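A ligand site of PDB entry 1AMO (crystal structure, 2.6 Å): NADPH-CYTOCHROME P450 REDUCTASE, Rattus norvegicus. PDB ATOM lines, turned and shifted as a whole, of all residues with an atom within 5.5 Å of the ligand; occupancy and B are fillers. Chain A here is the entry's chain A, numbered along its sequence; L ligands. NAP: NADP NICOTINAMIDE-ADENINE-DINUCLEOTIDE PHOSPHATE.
Residues that only touch the ligand: Val 411 (3.9 Å), Gly 471 (3.4 Å), Asn 572 (3.8 Å) and Met 573 (3.6 Å).
Hydrophobic or aromatic side chains that line the ligand: Val 411, Tyr 541 and Met 573.
14 residues have an atom within 4 Å of the ligand: Arg 235, Val 411, Gly 471, Thr 472, Cys 503, Arg 504, Ser 533, Arg 534, Lys 539, Tyr 541, Gln 543, Asn 572, Met 573 and Asp 576.
Along chain A the residues within 4 Å of the ligand span positions 235 to 576.
The nearest printed residue that does not touch the ligand is Pro 470 (4.003 Å).
O1X of the ligand lies within hydrogen-bond range of OH of Tyr 541, at 2.8 Å.
O of Cys 503 sits close to O3B of the ligand, at 3.3 Å.
O2N of the ligand sits at hydrogen-bond distance from N of Thr 472 (3.0 Å).
The guanidinium group (NE) of Arg 534 is in salt-bridge range of an oxygen (O2X) of the ligand.
O2A of the ligand is in salt-bridge range of NE of Arg 504, 3.5 Å away.
N6A of the ligand sits at hydrogen-bond distance from OD2 of Asp 576.
An oxygen (O2N) of the ligand is in hydrogen-bond range of the side-chain hydroxyl of Thr 472, at 3.5 Å.
A nitrogen (N1A) of the ligand is in hydrogen-bond range of the side-chain amide nitrogen of Gln 543 (3.2 Å).
NH2 of Arg 235 lies within salt-bridge range of O1A of the ligand.
OG of Ser 533 is in hydrogen-bond range of O2X of the ligand (2.7 Å).
O2X of the ligand is in salt-bridge range of NZ of Lys 539 (2.9 Å).
N of Asn 572 is in hydrogen-bond range of OD2 of Asp 569 (3.0 Å).
N of Ser 533 is in hydrogen-bond range of O of Arg 504, 3.5 Å away.
O of Gly 502 is in hydrogen-bond range of N of Gly 471 (3.0 Å).
The backbone carbonyl oxygen of Arg 504 is in hydrogen-bond range of the backbone NH of Arg 534, 3.0 Å away.
The backbone carbonyl oxygen (O) of Val 540 lies close to the backbone NH (N) of Ser 533 (3.3 Å).
N of Met 573 is in hydrogen-bond range of OD2 of Asp 569 (3.0 Å).
The backbone NH of Cys 503 sits at hydrogen-bond distance from the backbone carbonyl oxygen of Ala 531 (3.0 Å).
N of Ser 533 lies within hydrogen-bond range of O of Cys 503 (3.0 Å).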
ATOM      1  N   ARG A 235      27.281  25.412 -31.959  1.00  0.00           N
ATOM      2  CA  ARG A 235      28.626  25.404 -31.405  1.00  0.00           C
ATOM      3  C   ARG A 235      29.655  25.125 -32.491  1.00  0.00           C
ATOM      4  O   ARG A 235      29.291  24.944 -33.662  1.00  0.00           O
ATOM      5  CB  ARG A 235      28.760  24.341 -30.299  1.00  0.00           C
ATOM      6  CG  ARG A 235      28.233  24.767 -28.939  1.00  0.00           C
ATOM      7  CD  ARG A 235      28.605  23.748 -27.857  1.00  0.00           C
ATOM      8  NE  ARG A 235      27.932  22.467 -28.054  1.00  0.00           N
ATOM      9  CZ  ARG A 235      28.390  21.306 -27.591  1.00  0.00           C
ATOM     10  NH1 ARG A 235      29.524  21.261 -26.902  1.00  0.00           N
ATOM     11  NH2 ARG A 235      27.705  20.187 -27.807  1.00  0.00           N
ATOM     12  N   LEU A 237      33.011  22.659 -32.914  1.00  0.00           N
ATOM     13  CA  LEU A 237      33.921  21.663 -32.408  1.00  0.00           C
ATOM     14  C   LEU A 237      34.861  21.411 -33.556  1.00  0.00           C
ATOM     15  O   LEU A 237      34.406  21.257 -34.699  1.00  0.00           O
ATOM     16  CB  LEU A 237      33.162  20.409 -31.977  1.00  0.00           C
ATOM     17  CG  LEU A 237      32.223  20.651 -30.769  1.00  0.00           C
ATOM     18  CD1 LEU A 237      30.838  20.989 -31.252  1.00  0.00           C
ATOM     19  CD2 LEU A 237      32.166  19.432 -29.859  1.00  0.00           C
ATOM     20  N   VAL A 411      36.344  21.863 -28.283  1.00  0.00           N
ATOM     21  CA  VAL A 411      35.170  22.694 -28.497  1.00  0.00           C
ATOM     22  C   VAL A 411      35.624  24.123 -28.214  1.00  0.00           C
ATOM     23  O   VAL A 411      36.222  24.409 -27.176  1.00  0.00           O
ATOM     24  CB  VAL A 411      34.011  22.285 -27.549  1.00  0.00           C
ATOM     25  CG1 VAL A 411      34.499  22.251 -26.116  1.00  0.00           C
ATOM     26  CG2 VAL A 411      32.855  23.235 -27.691  1.00  0.00           C
ATOM     27  N   PRO A 470      31.311  10.967 -23.334  1.00  0.00           N
ATOM     28  CA  PRO A 470      30.335  11.873 -23.942  1.00  0.00           C
ATOM     29  C   PRO A 470      30.909  13.263 -24.237  1.00  0.00           C
ATOM     30  O   PRO A 470      31.571  13.867 -23.395  1.00  0.00           O
ATOM     31  CB  PRO A 470      29.231  11.935 -22.880  1.00  0.00           C
ATOM     32  CG  PRO A 470      29.983  11.827 -21.631  1.00  0.00           C
ATOM     33  CD  PRO A 470      31.002  10.737 -21.913  1.00  0.00           C
ATOM     34  N   GLY A 471      30.626  13.777 -25.441  1.00  0.00           N
ATOM     35  CA  GLY A 471      31.109  15.090 -25.828  1.00  0.00           C
ATOM     36  C   GLY A 471      32.533  15.053 -26.332  1.00  0.00           C
ATOM     37  O   GLY A 471      32.916  14.142 -27.090  1.00  0.00           O
ATOM     38  N   THR A 472      33.330  16.047 -25.954  1.00  0.00           N
ATOM     39  CA  THR A 472      34.721  16.083 -26.378  1.00  0.00           C
ATOM     40  C   THR A 472      35.528  15.058 -25.615  1.00  0.00           C
ATOM     41  O   THR A 472      36.728  14.939 -25.825  1.00  0.00           O
ATOM     42  CB  THR A 472      35.339  17.453 -26.202  1.00  0.00           C
ATOM     43  OG1 THR A 472      35.033  17.949 -24.895  1.00  0.00           O
ATOM     44  CG2 THR A 472      34.828  18.413 -27.258  1.00  0.00           C
ATOM     45  N   GLY A 473      34.863  14.328 -24.737  1.00  0.00           N
ATOM     46  CA  GLY A 473      35.529  13.285 -23.978  1.00  0.00           C
ATOM     47  C   GLY A 473      35.764  12.054 -24.842  1.00  0.00           C
ATOM     48  O   GLY A 473      36.148  11.008 -24.330  1.00  0.00           O
ATOM     49  N   GLY A 502      28.161  10.050 -26.353  1.00  0.00           N
ATOM     50  CA  GLY A 502      26.958  10.832 -26.148  1.00  0.00           C
ATOM     51  C   GLY A 502      27.105  12.220 -26.763  1.00  0.00           C
ATOM     52  O   GLY A 502      28.197  12.786 -26.801  1.00  0.00           O
ATOM     53  N   CYS A 503      26.001  12.749 -27.278  1.00  0.00           N
ATOM     54  CA  CYS A 503      25.971  14.068 -27.889  1.00  0.00           C
ATOM     55  C   CYS A 503      24.531  14.557 -27.882  1.00  0.00           C
ATOM     56  O   CYS A 503      23.615  13.811 -27.531  1.00  0.00           O
ATOM     57  CB  CYS A 503      26.516  14.041 -29.325  1.00  0.00           C
ATOM     58  SG  CYS A 503      25.526  13.192 -30.558  1.00  0.00           S
ATOM     59  N   ARG A 504      24.327  15.808 -28.278  1.00  0.00           N
ATOM     60  CA  ARG A 504      22.995  16.399 -28.287  1.00  0.00           C
ATOM     61  C   ARG A 504      22.051  15.822 -29.336  1.00  0.00           C
ATOM     62  O   ARG A 504      21.126  15.073 -29.006  1.00  0.00           O
ATOM     63  CB  ARG A 504      23.116  17.914 -28.423  1.00  0.00           C
ATOM     64  CG  ARG A 504      23.775  18.569 -27.210  1.00  0.00           C
ATOM     65  CD  ARG A 504      24.289  19.952 -27.536  1.00  0.00           C
ATOM     66  NE  ARG A 504      24.874  20.618 -26.376  1.00  0.00           N
ATOM     67  CZ  ARG A 504      24.967  21.939 -26.253  1.00  0.00           C
ATOM     68  NH1 ARG A 504      24.514  22.749 -27.209  1.00  0.00           N
ATOM     69  NH2 ARG A 504      25.499  22.466 -25.155  1.00  0.00           N
ATOM     70  N   ALA A 531      24.215   8.046 -27.040  1.00  0.00           N
ATOM     71  CA  ALA A 531      23.037   8.616 -26.405  1.00  0.00           C
ATOM     72  C   ALA A 531      22.845  10.025 -26.930  1.00  0.00           C
ATOM     73  O   ALA A 531      23.747  10.851 -26.820  1.00  0.00           O
ATOM     74  CB  ALA A 531      23.223   8.655 -24.900  1.00  0.00           C
ATOM     75  N   SER A 533      21.023  13.032 -26.213  1.00  0.00           N
ATOM     76  CA  SER A 533      20.321  13.670 -25.106  1.00  0.00           C
ATOM     77  C   SER A 533      19.239  14.671 -25.446  1.00  0.00           C
ATOM     78  O   SER A 533      18.409  15.004 -24.584  1.00  0.00           O
ATOM     79  CB  SER A 533      21.354  14.354 -24.204  1.00  0.00           C
ATOM     80  OG  SER A 533      21.964  15.422 -24.890  1.00  0.00           O
ATOM     81  N   ARG A 534      19.222  15.165 -26.683  1.00  0.00           N
ATOM     82  CA  ARG A 534      18.224  16.168 -27.061  1.00  0.00           C
ATOM     83  C   ARG A 534      17.288  15.801 -28.198  1.00  0.00           C
ATOM     84  O   ARG A 534      16.520  16.649 -28.662  1.00  0.00           O
ATOM     85  CB  ARG A 534      18.927  17.500 -27.353  1.00  0.00           C
ATOM     86  CG  ARG A 534      19.693  18.070 -26.148  1.00  0.00           C
ATOM     87  CD  ARG A 534      20.360  19.422 -26.451  1.00  0.00           C
ATOM     88  NE  ARG A 534      20.822  20.075 -25.214  1.00  0.00           N
ATOM     89  CZ  ARG A 534      20.834  21.384 -25.023  1.00  0.00           C
ATOM     90  NH1 ARG A 534      20.438  22.210 -25.967  1.00  0.00           N
ATOM     91  NH2 ARG A 534      21.196  21.876 -23.840  1.00  0.00           N
ATOM     92  N   LYS A 539      15.896  13.552 -21.399  1.00  0.00           N
ATOM     93  CA  LYS A 539      17.327  13.506 -21.693  1.00  0.00           C
ATOM     94  C   LYS A 539      17.894  12.095 -21.599  1.00  0.00           C
ATOM     95  O   LYS A 539      17.726  11.427 -20.588  1.00  0.00           O
ATOM     96  CB  LYS A 539      18.096  14.430 -20.745  1.00  0.00           C
ATOM     97  CG  LYS A 539      18.011  15.889 -21.146  1.00  0.00           C
ATOM     98  CD  LYS A 539      18.889  16.728 -20.277  1.00  0.00           C
ATOM     99  CE  LYS A 539      18.941  18.151 -20.765  1.00  0.00           C
ATOM    100  NZ  LYS A 539      19.140  18.217 -22.230  1.00  0.00           N
ATOM    101  N   VAL A 540      18.444  11.634 -22.689  1.00  0.00           N
ATOM    102  CA  VAL A 540      19.127  10.338 -22.651  1.00  0.00           C
ATOM    103  C   VAL A 540      20.629  10.560 -22.561  1.00  0.00           C
ATOM    104  O   VAL A 540      21.227  11.231 -23.411  1.00  0.00           O
ATOM    105  CB  VAL A 540      18.777   9.539 -23.907  1.00  0.00           C
ATOM    106  CG1 VAL A 540      19.340   8.117 -23.883  1.00  0.00           C
ATOM    107  CG2 VAL A 540      17.269   9.388 -24.116  1.00  0.00           C
ATOM    108  N   TYR A 541      21.191   9.986 -21.510  1.00  0.00           N
ATOM    109  CA  TYR A 541      22.628  10.087 -21.213  1.00  0.00           C
ATOM    110  C   TYR A 541      23.284   8.711 -21.296  1.00  0.00           C
ATOM    111  O   TYR A 541      22.603   7.665 -21.262  1.00  0.00           O
ATOM    112  CB  TYR A 541      22.803  10.631 -19.793  1.00  0.00           C
ATOM    113  CG  TYR A 541      22.446  12.119 -19.631  1.00  0.00           C
ATOM    114  CD1 TYR A 541      22.373  12.960 -20.757  1.00  0.00           C
ATOM    115  CD2 TYR A 541      22.199  12.631 -18.363  1.00  0.00           C
ATOM    116  CE1 TYR A 541      22.062  14.316 -20.584  1.00  0.00           C
ATOM    117  CE2 TYR A 541      21.888  13.987 -18.201  1.00  0.00           C
ATOM    118  CZ  TYR A 541      21.824  14.831 -19.306  1.00  0.00           C
ATOM    119  OH  TYR A 541      21.553  16.156 -19.143  1.00  0.00           O
ATOM    120  N   VAL A 542      24.599   8.726 -21.403  1.00  0.00           N
ATOM    121  CA  VAL A 542      25.404   7.494 -21.501  1.00  0.00           C
ATOM    122  C   VAL A 542      25.177   6.603 -20.284  1.00  0.00           C
ATOM    123  O   VAL A 542      25.306   5.374 -20.370  1.00  0.00           O
ATOM    124  CB  VAL A 542      26.892   7.826 -21.591  1.00  0.00           C
ATOM    125  CG1 VAL A 542      27.247   8.556 -22.876  1.00  0.00           C
ATOM    126  CG2 VAL A 542      27.360   8.730 -20.441  1.00  0.00           C
ATOM    127  N   GLN A 543      24.825   7.128 -19.108  1.00  0.00           N
ATOM    128  CA  GLN A 543      24.599   6.278 -17.940  1.00  0.00           C
ATOM    129  C   GLN A 543      23.413   5.365 -18.198  1.00  0.00           C
ATOM    130  O   GLN A 543      23.366   4.233 -17.717  1.00  0.00           O
ATOM    131  CB  GLN A 543      24.280   7.092 -16.682  1.00  0.00           C
ATOM    132  CG  GLN A 543      25.191   8.251 -16.399  1.00  0.00           C
ATOM    133  CD  GLN A 543      24.807   9.474 -17.170  1.00  0.00           C
ATOM    134  OE1 GLN A 543      25.217   9.648 -18.309  1.00  0.00           O
ATOM    135  NE2 GLN A 543      23.997  10.331 -16.554  1.00  0.00           N
ATOM    136  N   ASP A 569      33.711  15.585 -18.705  1.00  0.00           N
ATOM    137  CA  ASP A 569      33.233  16.470 -17.640  1.00  0.00           C
ATOM    138  C   ASP A 569      33.397  15.840 -16.250  1.00  0.00           C
ATOM    139  O   ASP A 569      32.935  14.730 -16.001  1.00  0.00           O
ATOM    140  CB  ASP A 569      31.754  16.794 -17.926  1.00  0.00           C
ATOM    141  CG  ASP A 569      31.084  17.543 -16.817  1.00  0.00           C
ATOM    142  OD1 ASP A 569      31.514  18.676 -16.527  1.00  0.00           O
ATOM    143  OD2 ASP A 569      30.114  17.010 -16.246  1.00  0.00           O
ATOM    144  N   ASN A 572      29.749  16.794 -13.296  1.00  0.00           N
ATOM    145  CA  ASN A 572      28.575  15.926 -13.292  1.00  0.00           C
ATOM    146  C   ASN A 572      28.699  14.541 -13.920  1.00  0.00           C
ATOM    147  O   ASN A 572      28.561  13.528 -13.231  1.00  0.00           O
ATOM    148  CB  ASN A 572      27.380  16.648 -13.908  1.00  0.00           C
ATOM    149  CG  ASN A 572      26.980  17.886 -13.108  1.00  0.00           C
ATOM    150  OD1 ASN A 572      26.853  18.981 -13.663  1.00  0.00           O
ATOM    151  ND2 ASN A 572      26.772  17.715 -11.804  1.00  0.00           N
ATOM    152  N   MET A 573      28.914  14.496 -15.235  1.00  0.00           N
ATOM    153  CA  MET A 573      28.999  13.225 -15.943  1.00  0.00           C
ATOM    154  C   MET A 573      29.809  12.159 -15.240  1.00  0.00           C
ATOM    155  O   MET A 573      29.294  11.086 -14.942  1.00  0.00           O
ATOM    156  CB  MET A 573      29.529  13.442 -17.358  1.00  0.00           C
ATOM    157  CG  MET A 573      29.605  12.178 -18.196  1.00  0.00           C
ATOM    158  SD  MET A 573      31.160  11.285 -18.023  1.00  0.00           S
ATOM    159  CE  MET A 573      32.235  12.376 -18.868  1.00  0.00           C
ATOM    160  N   ASP A 576      28.271  10.817 -12.069  1.00  0.00           N
ATOM    161  CA  ASP A 576      27.006  10.162 -12.367  1.00  0.00           C
ATOM    162  C   ASP A 576      27.319   8.755 -12.839  1.00  0.00           C
ATOM    163  O   ASP A 576      26.717   7.793 -12.372  1.00  0.00           O
ATOM    164  CB  ASP A 576      26.223  10.903 -13.431  1.00  0.00           C
ATOM    165  CG  ASP A 576      25.468  12.096 -12.871  1.00  0.00           C
ATOM    166  OD1 ASP A 576      25.351  12.209 -11.633  1.00  0.00           O
ATOM    167  OD2 ASP A 576      24.993  12.932 -13.667  1.00  0.00           O
HETATM  168  PA  NAP L   1      28.596  18.686 -24.284  1.00  0.00           P
HETATM  169  O1A NAP L   1      29.170  18.314 -25.613  1.00  0.00           O
HETATM  170  O2A NAP L   1      27.422  19.569 -24.228  1.00  0.00           O
HETATM  171  O5B NAP L   1      28.192  17.415 -23.434  1.00  0.00           O
HETATM  172  C5B NAP L   1      28.119  16.152 -24.096  1.00  0.00           C
HETATM  173  C4B NAP L   1      26.835  15.388 -23.765  1.00  0.00           C
HETATM  174  O4B NAP L   1      26.722  15.014 -22.380  1.00  0.00           O
HETATM  175  C3B NAP L   1      25.514  16.045 -24.084  1.00  0.00           C
HETATM  176  O3B NAP L   1      24.720  15.021 -24.652  1.00  0.00           O
HETATM  177  C2B NAP L   1      24.987  16.512 -22.733  1.00  0.00           C
HETATM  178  O2B NAP L   1      23.556  16.631 -22.769  1.00  0.00           O
HETATM  179  C1B NAP L   1      25.419  15.333 -21.891  1.00  0.00           C
HETATM  180  N9A NAP L   1      25.530  15.497 -20.416  1.00  0.00           N
HETATM  181  C8A NAP L   1      25.318  16.537 -19.603  1.00  0.00           C
HETATM  182  N7A NAP L   1      25.317  16.142 -18.296  1.00  0.00           N
HETATM  183  C5A NAP L   1      25.539  14.835 -18.360  1.00  0.00           C
HETATM  184  C6A NAP L   1      25.615  13.953 -17.295  1.00  0.00           C
HETATM  185  N6A NAP L   1      25.326  14.278 -16.059  1.00  0.00           N
HETATM  186  N1A NAP L   1      25.886  12.680 -17.588  1.00  0.00           N
HETATM  187  C2A NAP L   1      26.077  12.297 -18.856  1.00  0.00           C
HETATM  188  N3A NAP L   1      25.988  13.113 -19.893  1.00  0.00           N
HETATM  189  C4A NAP L   1      25.710  14.416 -19.660  1.00  0.00           C
HETATM  190  O3  NAP L   1      29.829  19.207 -23.399  1.00  0.00           O
HETATM  191  PN  NAP L   1      31.308  19.350 -23.910  1.00  0.00           P
HETATM  192  O1N NAP L   1      31.509  20.773 -24.164  1.00  0.00           O
HETATM  193  O2N NAP L   1      31.586  18.318 -24.931  1.00  0.00           O
HETATM  194  O5D NAP L   1      31.991  18.986 -22.534  1.00  0.00           O
HETATM  195  P2B NAP L   1      22.786  17.955 -22.569  1.00  0.00           P
HETATM  196  O1X NAP L   1      22.379  17.936 -21.149  1.00  0.00           O
HETATM  197  O2X NAP L   1      21.709  17.787 -23.558  1.00  0.00           O
HETATM  198  O3X NAP L   1      23.795  18.975 -22.945  1.00  0.00           O
